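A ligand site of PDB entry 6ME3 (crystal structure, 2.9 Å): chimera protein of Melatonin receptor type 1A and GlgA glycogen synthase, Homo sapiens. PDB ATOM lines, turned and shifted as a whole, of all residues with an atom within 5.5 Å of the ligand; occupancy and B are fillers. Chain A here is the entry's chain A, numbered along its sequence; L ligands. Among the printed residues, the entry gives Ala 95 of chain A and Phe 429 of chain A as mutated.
An oxygen (O2) of the ligand is in hydrogen-bond range of the side-chain amide nitrogen (ND2) of Asn 153 (2.8 Å). The side-chain amide nitrogen (NE2) of Gln 172 is in hydrogen-bond range of an oxygen (O1) of the ligand (2.8 Å).
NE2 of Gln 172 is in hydrogen-bond range of O of Leu 432 (3.2 Å). The side-chain hydroxyl of Tyr 72 is in hydrogen-bond range of the backbone carbonyl oxygen of Tyr 463 (3.2 Å). ND2 of Asn 433 lies within hydrogen-bond range of O of Phe 429 (2.9 Å).
Ala 95 touches the ligand (O to C18, 3.3 Å). O of Met 98 touches C13 of the ligand, at 3.7 Å. CA of Gly 99 touches C18 of the ligand, at 3.3 Å. Val 102 touches the ligand. CG1 of Val 150 touches C19 of the ligand, at 3.9 Å. CD2 of Leu 159 touches C19 of the ligand, at 3.8 Å. Thr 169 touches the ligand. CD2 of Phe 170 touches O1 of the ligand (3.5 Å). Val 182 touches the ligand. Leu 432 touches the ligand. OD1 of Asn 433 touches C4 of the ligand, at 3.7 Å. Tyr 459 touches the ligand. CB of Ala 462 touches C11 of the ligand, at 3.8 Å. CE1 of Tyr 463 touches C12 of the ligand (3.6 Å). Hydrophobic or aromatic side chains within 4 Å of the ligand: Met 98, Val 102, Val 150, Leu 159, Phe 170, Val 182, Leu 432, Tyr 459, Ala 462 and Tyr 463. 16 residues have an atom within 4 Å of the ligand: Ala 95, Met 98, Gly 99, Val 102, Val 150, Asn 153, Leu 159, Thr 169, Phe 170, Gln 172, Val 182, Leu 432, Asn 433, Tyr 459, Ala 462 and Tyr 463.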
ATOM      1  N   TYR A  72       8.397  10.836  14.752  1.00  0.00           N
ATOM      2  CA  TYR A  72       8.529  11.549  13.481  1.00  0.00           C
ATOM      3  C   TYR A  72       7.463  12.642  13.272  1.00  0.00           C
ATOM      4  O   TYR A  72       7.869  13.731  12.850  1.00  0.00           O
ATOM      5  CB  TYR A  72       8.532  10.610  12.273  1.00  0.00           C
ATOM      6  CG  TYR A  72       9.810   9.822  12.071  1.00  0.00           C
ATOM      7  CD1 TYR A  72      10.912  10.030  12.902  1.00  0.00           C
ATOM      8  CD2 TYR A  72       9.928   8.906  11.036  1.00  0.00           C
ATOM      9  CE1 TYR A  72      12.095   9.308  12.721  1.00  0.00           C
ATOM     10  CE2 TYR A  72      11.118   8.194  10.836  1.00  0.00           C
ATOM     11  CZ  TYR A  72      12.192   8.394  11.680  1.00  0.00           C
ATOM     12  OH  TYR A  72      13.351   7.697  11.494  1.00  0.00           O
ATOM     13  N   ALA A  95      12.475  11.174  22.088  1.00  0.00           N
ATOM     14  CA  ALA A  95      13.903  10.930  21.895  1.00  0.00           C
ATOM     15  C   ALA A  95      14.253   9.463  22.223  1.00  0.00           C
ATOM     16  O   ALA A  95      14.973   8.823  21.455  1.00  0.00           O
ATOM     17  CB  ALA A  95      14.722  11.874  22.763  1.00  0.00           C
ATOM     18  N   PHE A  96      13.682   8.931  23.335  1.00  0.00           N
ATOM     19  CA  PHE A  96      13.854   7.562  23.833  1.00  0.00           C
ATOM     20  C   PHE A  96      13.390   6.509  22.821  1.00  0.00           C
ATOM     21  O   PHE A  96      14.147   5.594  22.520  1.00  0.00           O
ATOM     22  CB  PHE A  96      13.099   7.390  25.177  1.00  0.00           C
ATOM     23  CG  PHE A  96      13.287   6.056  25.864  1.00  0.00           C
ATOM     24  CD1 PHE A  96      14.407   5.817  26.659  1.00  0.00           C
ATOM     25  CD2 PHE A  96      12.307   5.067  25.788  1.00  0.00           C
ATOM     26  CE1 PHE A  96      14.559   4.588  27.317  1.00  0.00           C
ATOM     27  CE2 PHE A  96      12.461   3.851  26.465  1.00  0.00           C
ATOM     28  CZ  PHE A  96      13.584   3.614  27.214  1.00  0.00           C
ATOM     29  N   MET A  98      12.965   6.827  19.631  1.00  0.00           N
ATOM     30  CA  MET A  98      13.846   6.910  18.456  1.00  0.00           C
ATOM     31  C   MET A  98      15.132   6.110  18.697  1.00  0.00           C
ATOM     32  O   MET A  98      15.703   5.567  17.745  1.00  0.00           O
ATOM     33  CB  MET A  98      14.201   8.354  18.132  1.00  0.00           C
ATOM     34  CG  MET A  98      13.277   8.974  17.143  1.00  0.00           C
ATOM     35  SD  MET A  98      13.743  10.698  16.935  1.00  0.00           S
ATOM     36  CE  MET A  98      12.637  11.174  15.722  1.00  0.00           C
ATOM     37  N   GLY A  99      15.545   6.034  19.966  1.00  0.00           N
ATOM     38  CA  GLY A  99      16.686   5.236  20.388  1.00  0.00           C
ATOM     39  C   GLY A  99      16.364   3.761  20.308  1.00  0.00           C
ATOM     40  O   GLY A  99      17.066   3.013  19.612  1.00  0.00           O
ATOM     41  N   VAL A 102      16.068   2.629  16.335  1.00  0.00           N
ATOM     42  CA  VAL A 102      17.333   2.601  15.610  1.00  0.00           C
ATOM     43  C   VAL A 102      18.351   1.578  16.213  1.00  0.00           C
ATOM     44  O   VAL A 102      19.077   0.957  15.430  1.00  0.00           O
ATOM     45  CB  VAL A 102      17.905   4.044  15.506  1.00  0.00           C
ATOM     46  CG1 VAL A 102      19.439   4.109  15.479  1.00  0.00           C
ATOM     47  CG2 VAL A 102      17.315   4.753  14.301  1.00  0.00           C
ATOM     48  N   ILE A 103      18.379   1.382  17.544  1.00  0.00           N
ATOM     49  CA  ILE A 103      19.330   0.415  18.144  1.00  0.00           C
ATOM     50  C   ILE A 103      18.769  -1.021  17.984  1.00  0.00           C
ATOM     51  O   ILE A 103      19.522  -1.960  17.706  1.00  0.00           O
ATOM     52  CB  ILE A 103      19.712   0.768  19.628  1.00  0.00           C
ATOM     53  CG1 ILE A 103      20.327   2.207  19.743  1.00  0.00           C
ATOM     54  CG2 ILE A 103      20.646  -0.260  20.279  1.00  0.00           C
ATOM     55  CD1 ILE A 103      21.625   2.534  18.867  1.00  0.00           C
ATOM     56  N   ALA A 149      20.465  -0.430  26.812  1.00  0.00           N
ATOM     57  CA  ALA A 149      21.383   0.526  26.190  1.00  0.00           C
ATOM     58  C   ALA A 149      20.800   1.939  26.100  1.00  0.00           C
ATOM     59  O   ALA A 149      21.550   2.904  26.256  1.00  0.00           O
ATOM     60  CB  ALA A 149      21.748   0.038  24.792  1.00  0.00           C
ATOM     61  N   VAL A 150      19.486   2.072  25.830  1.00  0.00           N
ATOM     62  CA  VAL A 150      18.813   3.372  25.674  1.00  0.00           C
ATOM     63  C   VAL A 150      18.414   3.952  27.048  1.00  0.00           C
ATOM     64  O   VAL A 150      18.677   5.137  27.284  1.00  0.00           O
ATOM     65  CB  VAL A 150      17.605   3.299  24.696  1.00  0.00           C
ATOM     66  CG1 VAL A 150      17.012   4.691  24.457  1.00  0.00           C
ATOM     67  CG2 VAL A 150      17.995   2.663  23.362  1.00  0.00           C
ATOM     68  N   ASN A 153      20.221   6.828  29.340  1.00  0.00           N
ATOM     69  CA  ASN A 153      20.212   8.158  28.752  1.00  0.00           C
ATOM     70  C   ASN A 153      19.195   9.116  29.383  1.00  0.00           C
ATOM     71  O   ASN A 153      19.368  10.338  29.254  1.00  0.00           O
ATOM     72  CB  ASN A 153      19.946   8.058  27.265  1.00  0.00           C
ATOM     73  CG  ASN A 153      21.144   7.586  26.477  1.00  0.00           C
ATOM     74  OD1 ASN A 153      21.983   6.798  26.931  1.00  0.00           O
ATOM     75  ND2 ASN A 153      21.246   8.108  25.283  1.00  0.00           N
ATOM     76  N   LEU A 159      19.782  13.445  26.338  1.00  0.00           N
ATOM     77  CA  LEU A 159      18.702  13.623  25.364  1.00  0.00           C
ATOM     78  C   LEU A 159      18.242  15.051  25.418  1.00  0.00           C
ATOM     79  O   LEU A 159      17.851  15.509  26.494  1.00  0.00           O
ATOM     80  CB  LEU A 159      17.531  12.678  25.662  1.00  0.00           C
ATOM     81  CG  LEU A 159      17.781  11.181  25.580  1.00  0.00           C
ATOM     82  CD1 LEU A 159      16.684  10.416  26.284  1.00  0.00           C
ATOM     83  CD2 LEU A 159      17.953  10.726  24.136  1.00  0.00           C
ATOM     84  N   THR A 169      16.811  14.452  20.211  1.00  0.00           N
ATOM     85  CA  THR A 169      17.604  13.242  19.952  1.00  0.00           C
ATOM     86  C   THR A 169      18.798  13.106  20.960  1.00  0.00           C
ATOM     87  O   THR A 169      18.916  13.885  21.920  1.00  0.00           O
ATOM     88  CB  THR A 169      18.090  13.263  18.479  1.00  0.00           C
ATOM     89  OG1 THR A 169      18.591  11.971  18.110  1.00  0.00           O
ATOM     90  CG2 THR A 169      19.129  14.352  18.205  1.00  0.00           C
ATOM     91  N   PHE A 170      19.656  12.082  20.718  1.00  0.00           N
ATOM     92  CA  PHE A 170      20.849  11.832  21.515  1.00  0.00           C
ATOM     93  C   PHE A 170      21.923  12.859  21.166  1.00  0.00           C
ATOM     94  O   PHE A 170      22.458  12.835  20.051  1.00  0.00           O
ATOM     95  CB  PHE A 170      21.359  10.395  21.309  1.00  0.00           C
ATOM     96  CG  PHE A 170      22.705  10.081  21.936  1.00  0.00           C
ATOM     97  CD1 PHE A 170      22.816   9.815  23.293  1.00  0.00           C
ATOM     98  CD2 PHE A 170      23.859  10.067  21.160  1.00  0.00           C
ATOM     99  CE1 PHE A 170      24.051   9.515  23.870  1.00  0.00           C
ATOM    100  CE2 PHE A 170      25.105   9.785  21.745  1.00  0.00           C
ATOM    101  CZ  PHE A 170      25.184   9.512  23.093  1.00  0.00           C
ATOM    102  N   GLN A 172      25.456  14.191  20.947  1.00  0.00           N
ATOM    103  CA  GLN A 172      26.814  13.625  20.883  1.00  0.00           C
ATOM    104  C   GLN A 172      27.844  14.473  21.599  1.00  0.00           C
ATOM    105  O   GLN A 172      29.005  14.092  21.629  1.00  0.00           O
ATOM    106  CB  GLN A 172      27.252  13.452  19.431  1.00  0.00           C
ATOM    107  CG  GLN A 172      26.370  12.551  18.586  1.00  0.00           C
ATOM    108  CD  GLN A 172      26.695  12.668  17.118  1.00  0.00           C
ATOM    109  OE1 GLN A 172      27.221  13.681  16.630  1.00  0.00           O
ATOM    110  NE2 GLN A 172      26.360  11.627  16.362  1.00  0.00           N
ATOM    111  N   VAL A 182      28.451   4.211  22.159  1.00  0.00           N
ATOM    112  CA  VAL A 182      27.302   3.978  21.267  1.00  0.00           C
ATOM    113  C   VAL A 182      27.846   3.633  19.863  1.00  0.00           C
ATOM    114  O   VAL A 182      27.427   2.608  19.306  1.00  0.00           O
ATOM    115  CB  VAL A 182      26.299   5.173  21.273  1.00  0.00           C
ATOM    116  CG1 VAL A 182      25.241   5.034  20.170  1.00  0.00           C
ATOM    117  CG2 VAL A 182      25.638   5.311  22.636  1.00  0.00           C
ATOM    118  N   VAL A 183      28.803   4.436  19.336  1.00  0.00           N
ATOM    119  CA  VAL A 183      29.430   4.213  18.026  1.00  0.00           C
ATOM    120  C   VAL A 183      30.162   2.853  17.999  1.00  0.00           C
ATOM    121  O   VAL A 183      30.038   2.114  17.028  1.00  0.00           O
ATOM    122  CB  VAL A 183      30.387   5.380  17.602  1.00  0.00           C
ATOM    123  CG1 VAL A 183      31.139   5.055  16.315  1.00  0.00           C
ATOM    124  CG2 VAL A 183      29.622   6.698  17.452  1.00  0.00           C
ATOM    125  N   PHE A 429      23.446   5.225   8.126  1.00  0.00           N
ATOM    126  CA  PHE A 429      23.960   5.543   9.448  1.00  0.00           C
ATOM    127  C   PHE A 429      25.489   5.756   9.548  1.00  0.00           C
ATOM    128  O   PHE A 429      25.926   6.289  10.575  1.00  0.00           O
ATOM    129  CB  PHE A 429      23.507   4.473  10.444  1.00  0.00           C
ATOM    130  CG  PHE A 429      22.051   4.606  10.780  1.00  0.00           C
ATOM    131  CD1 PHE A 429      21.078   3.991   9.992  1.00  0.00           C
ATOM    132  CD2 PHE A 429      21.627   5.384  11.850  1.00  0.00           C
ATOM    133  CE1 PHE A 429      19.727   4.135  10.290  1.00  0.00           C
ATOM    134  CE2 PHE A 429      20.277   5.523  12.156  1.00  0.00           C
ATOM    135  CZ  PHE A 429      19.334   4.902  11.359  1.00  0.00           C
ATOM    136  N   LEU A 432      26.422   9.662  10.450  1.00  0.00           N
ATOM    137  CA  LEU A 432      26.043   9.974  11.838  1.00  0.00           C
ATOM    138  C   LEU A 432      27.077   9.486  12.839  1.00  0.00           C
ATOM    139  O   LEU A 432      27.466  10.263  13.707  1.00  0.00           O
ATOM    140  CB  LEU A 432      24.684   9.343  12.182  1.00  0.00           C
ATOM    141  CG  LEU A 432      23.954   9.938  13.390  1.00  0.00           C
ATOM    142  CD1 LEU A 432      22.988  10.992  12.943  1.00  0.00           C
ATOM    143  CD2 LEU A 432      23.187   8.875  14.130  1.00  0.00           C
ATOM    144  N   ASN A 433      27.501   8.218  12.717  1.00  0.00           N
ATOM    145  CA  ASN A 433      28.480   7.590  13.597  1.00  0.00           C
ATOM    146  C   ASN A 433      29.892   8.185  13.385  1.00  0.00           C
ATOM    147  O   ASN A 433      30.635   8.331  14.360  1.00  0.00           O
ATOM    148  CB  ASN A 433      28.480   6.082  13.400  1.00  0.00           C
ATOM    149  CG  ASN A 433      27.274   5.437  14.005  1.00  0.00           C
ATOM    150  OD1 ASN A 433      27.256   5.080  15.190  1.00  0.00           O
ATOM    151  ND2 ASN A 433      26.204   5.337  13.249  1.00  0.00           N
ATOM    152  N   GLY A 436      29.761  11.451  15.015  1.00  0.00           N
ATOM    153  CA  GLY A 436      29.735  11.090  16.418  1.00  0.00           C
ATOM    154  C   GLY A 436      31.127  10.988  17.012  1.00  0.00           C
ATOM    155  O   GLY A 436      31.391  11.571  18.066  1.00  0.00           O
ATOM    156  N   TYR A 459      21.387  13.255   9.585  1.00  0.00           N
ATOM    157  CA  TYR A 459      20.247  12.935  10.432  1.00  0.00           C
ATOM    158  C   TYR A 459      19.038  12.501   9.617  1.00  0.00           C
ATOM    159  O   TYR A 459      18.412  11.498   9.980  1.00  0.00           O
ATOM    160  CB  TYR A 459      19.888  14.097  11.383  1.00  0.00           C
ATOM    161  CG  TYR A 459      20.457  13.878  12.775  1.00  0.00           C
ATOM    162  CD1 TYR A 459      19.814  13.028  13.673  1.00  0.00           C
ATOM    163  CD2 TYR A 459      21.676  14.447  13.153  1.00  0.00           C
ATOM    164  CE1 TYR A 459      20.367  12.768  14.931  1.00  0.00           C
ATOM    165  CE2 TYR A 459      22.227  14.200  14.406  1.00  0.00           C
ATOM    166  CZ  TYR A 459      21.573  13.345  15.293  1.00  0.00           C
ATOM    167  OH  TYR A 459      22.142  13.060  16.511  1.00  0.00           O
ATOM    168  N   ALA A 462      19.350   9.006   7.953  1.00  0.00           N
ATOM    169  CA  ALA A 462      19.090   8.034   9.007  1.00  0.00           C
ATOM    170  C   ALA A 462      17.584   7.883   9.236  1.00  0.00           C
ATOM    171  O   ALA A 462      17.112   6.768   9.472  1.00  0.00           O
ATOM    172  CB  ALA A 462      19.769   8.468  10.289  1.00  0.00           C
ATOM    173  N   TYR A 463      16.832   9.014   9.179  1.00  0.00           N
ATOM    174  CA  TYR A 463      15.382   9.005   9.334  1.00  0.00           C
ATOM    175  C   TYR A 463      14.728   8.295   8.164  1.00  0.00           C
ATOM    176  O   TYR A 463      13.836   7.479   8.382  1.00  0.00           O
ATOM    177  CB  TYR A 463      14.803  10.424   9.465  1.00  0.00           C
ATOM    178  CG  TYR A 463      15.093  11.122  10.772  1.00  0.00           C
ATOM    179  CD1 TYR A 463      15.092  10.424  11.978  1.00  0.00           C
ATOM    180  CD2 TYR A 463      15.306  12.503  10.812  1.00  0.00           C
ATOM    181  CE1 TYR A 463      15.332  11.080  13.191  1.00  0.00           C
ATOM    182  CE2 TYR A 463      15.565  13.156  12.009  1.00  0.00           C
ATOM    183  CZ  TYR A 463      15.574  12.442  13.204  1.00  0.00           C
ATOM    184  OH  TYR A 463      15.821  13.082  14.385  1.00  0.00           O
HETATM  185  C1  LIG L   1      21.398   7.124  17.791  1.00  0.00           C
HETATM  186  C2  LIG L   1      22.509   8.038  18.284  1.00  0.00           C
HETATM  187  C3  LIG L   1      24.704   8.712  17.387  1.00  0.00           C
HETATM  188  O1  LIG L   1      24.589   9.892  17.744  1.00  0.00           O
HETATM  189  C4  LIG L   1      25.929   8.240  16.640  1.00  0.00           C
HETATM  190  O2  LIG L   1      20.838   6.300  23.208  1.00  0.00           O
HETATM  191  N1  LIG L   1      23.761   7.779  17.587  1.00  0.00           N
HETATM  192  C5  LIG L   1      20.110   6.867  22.198  1.00  0.00           C
HETATM  193  C6  LIG L   1      20.582   6.850  20.880  1.00  0.00           C
HETATM  194  C7  LIG L   1      19.857   7.419  19.823  1.00  0.00           C
HETATM  195  C8  LIG L   1      22.184   5.951  22.871  1.00  0.00           C
HETATM  196  C9  LIG L   1      19.751   9.193  15.676  1.00  0.00           C
HETATM  197  C10 LIG L   1      19.492   9.395  14.304  1.00  0.00           C
HETATM  198  C11 LIG L   1      18.276   8.983  13.721  1.00  0.00           C
HETATM  199  C12 LIG L   1      17.313   8.358  14.530  1.00  0.00           C
HETATM  200  C13 LIG L   1      17.584   8.125  15.895  1.00  0.00           C
HETATM  201  C14 LIG L   1      18.798   8.542  16.469  1.00  0.00           C
HETATM  202  N2  LIG L   1      18.106   8.462  18.886  1.00  0.00           N
HETATM  203  C15 LIG L   1      20.104   7.548  18.458  1.00  0.00           C
HETATM  204  C16 LIG L   1      19.043   8.255  17.891  1.00  0.00           C
HETATM  205  C17 LIG L   1      18.619   8.002  20.091  1.00  0.00           C
HETATM  206  C18 LIG L   1      18.135   8.032  21.406  1.00  0.00           C
HETATM  207  C19 LIG L   1      18.861   7.445  22.453  1.00  0.00           C
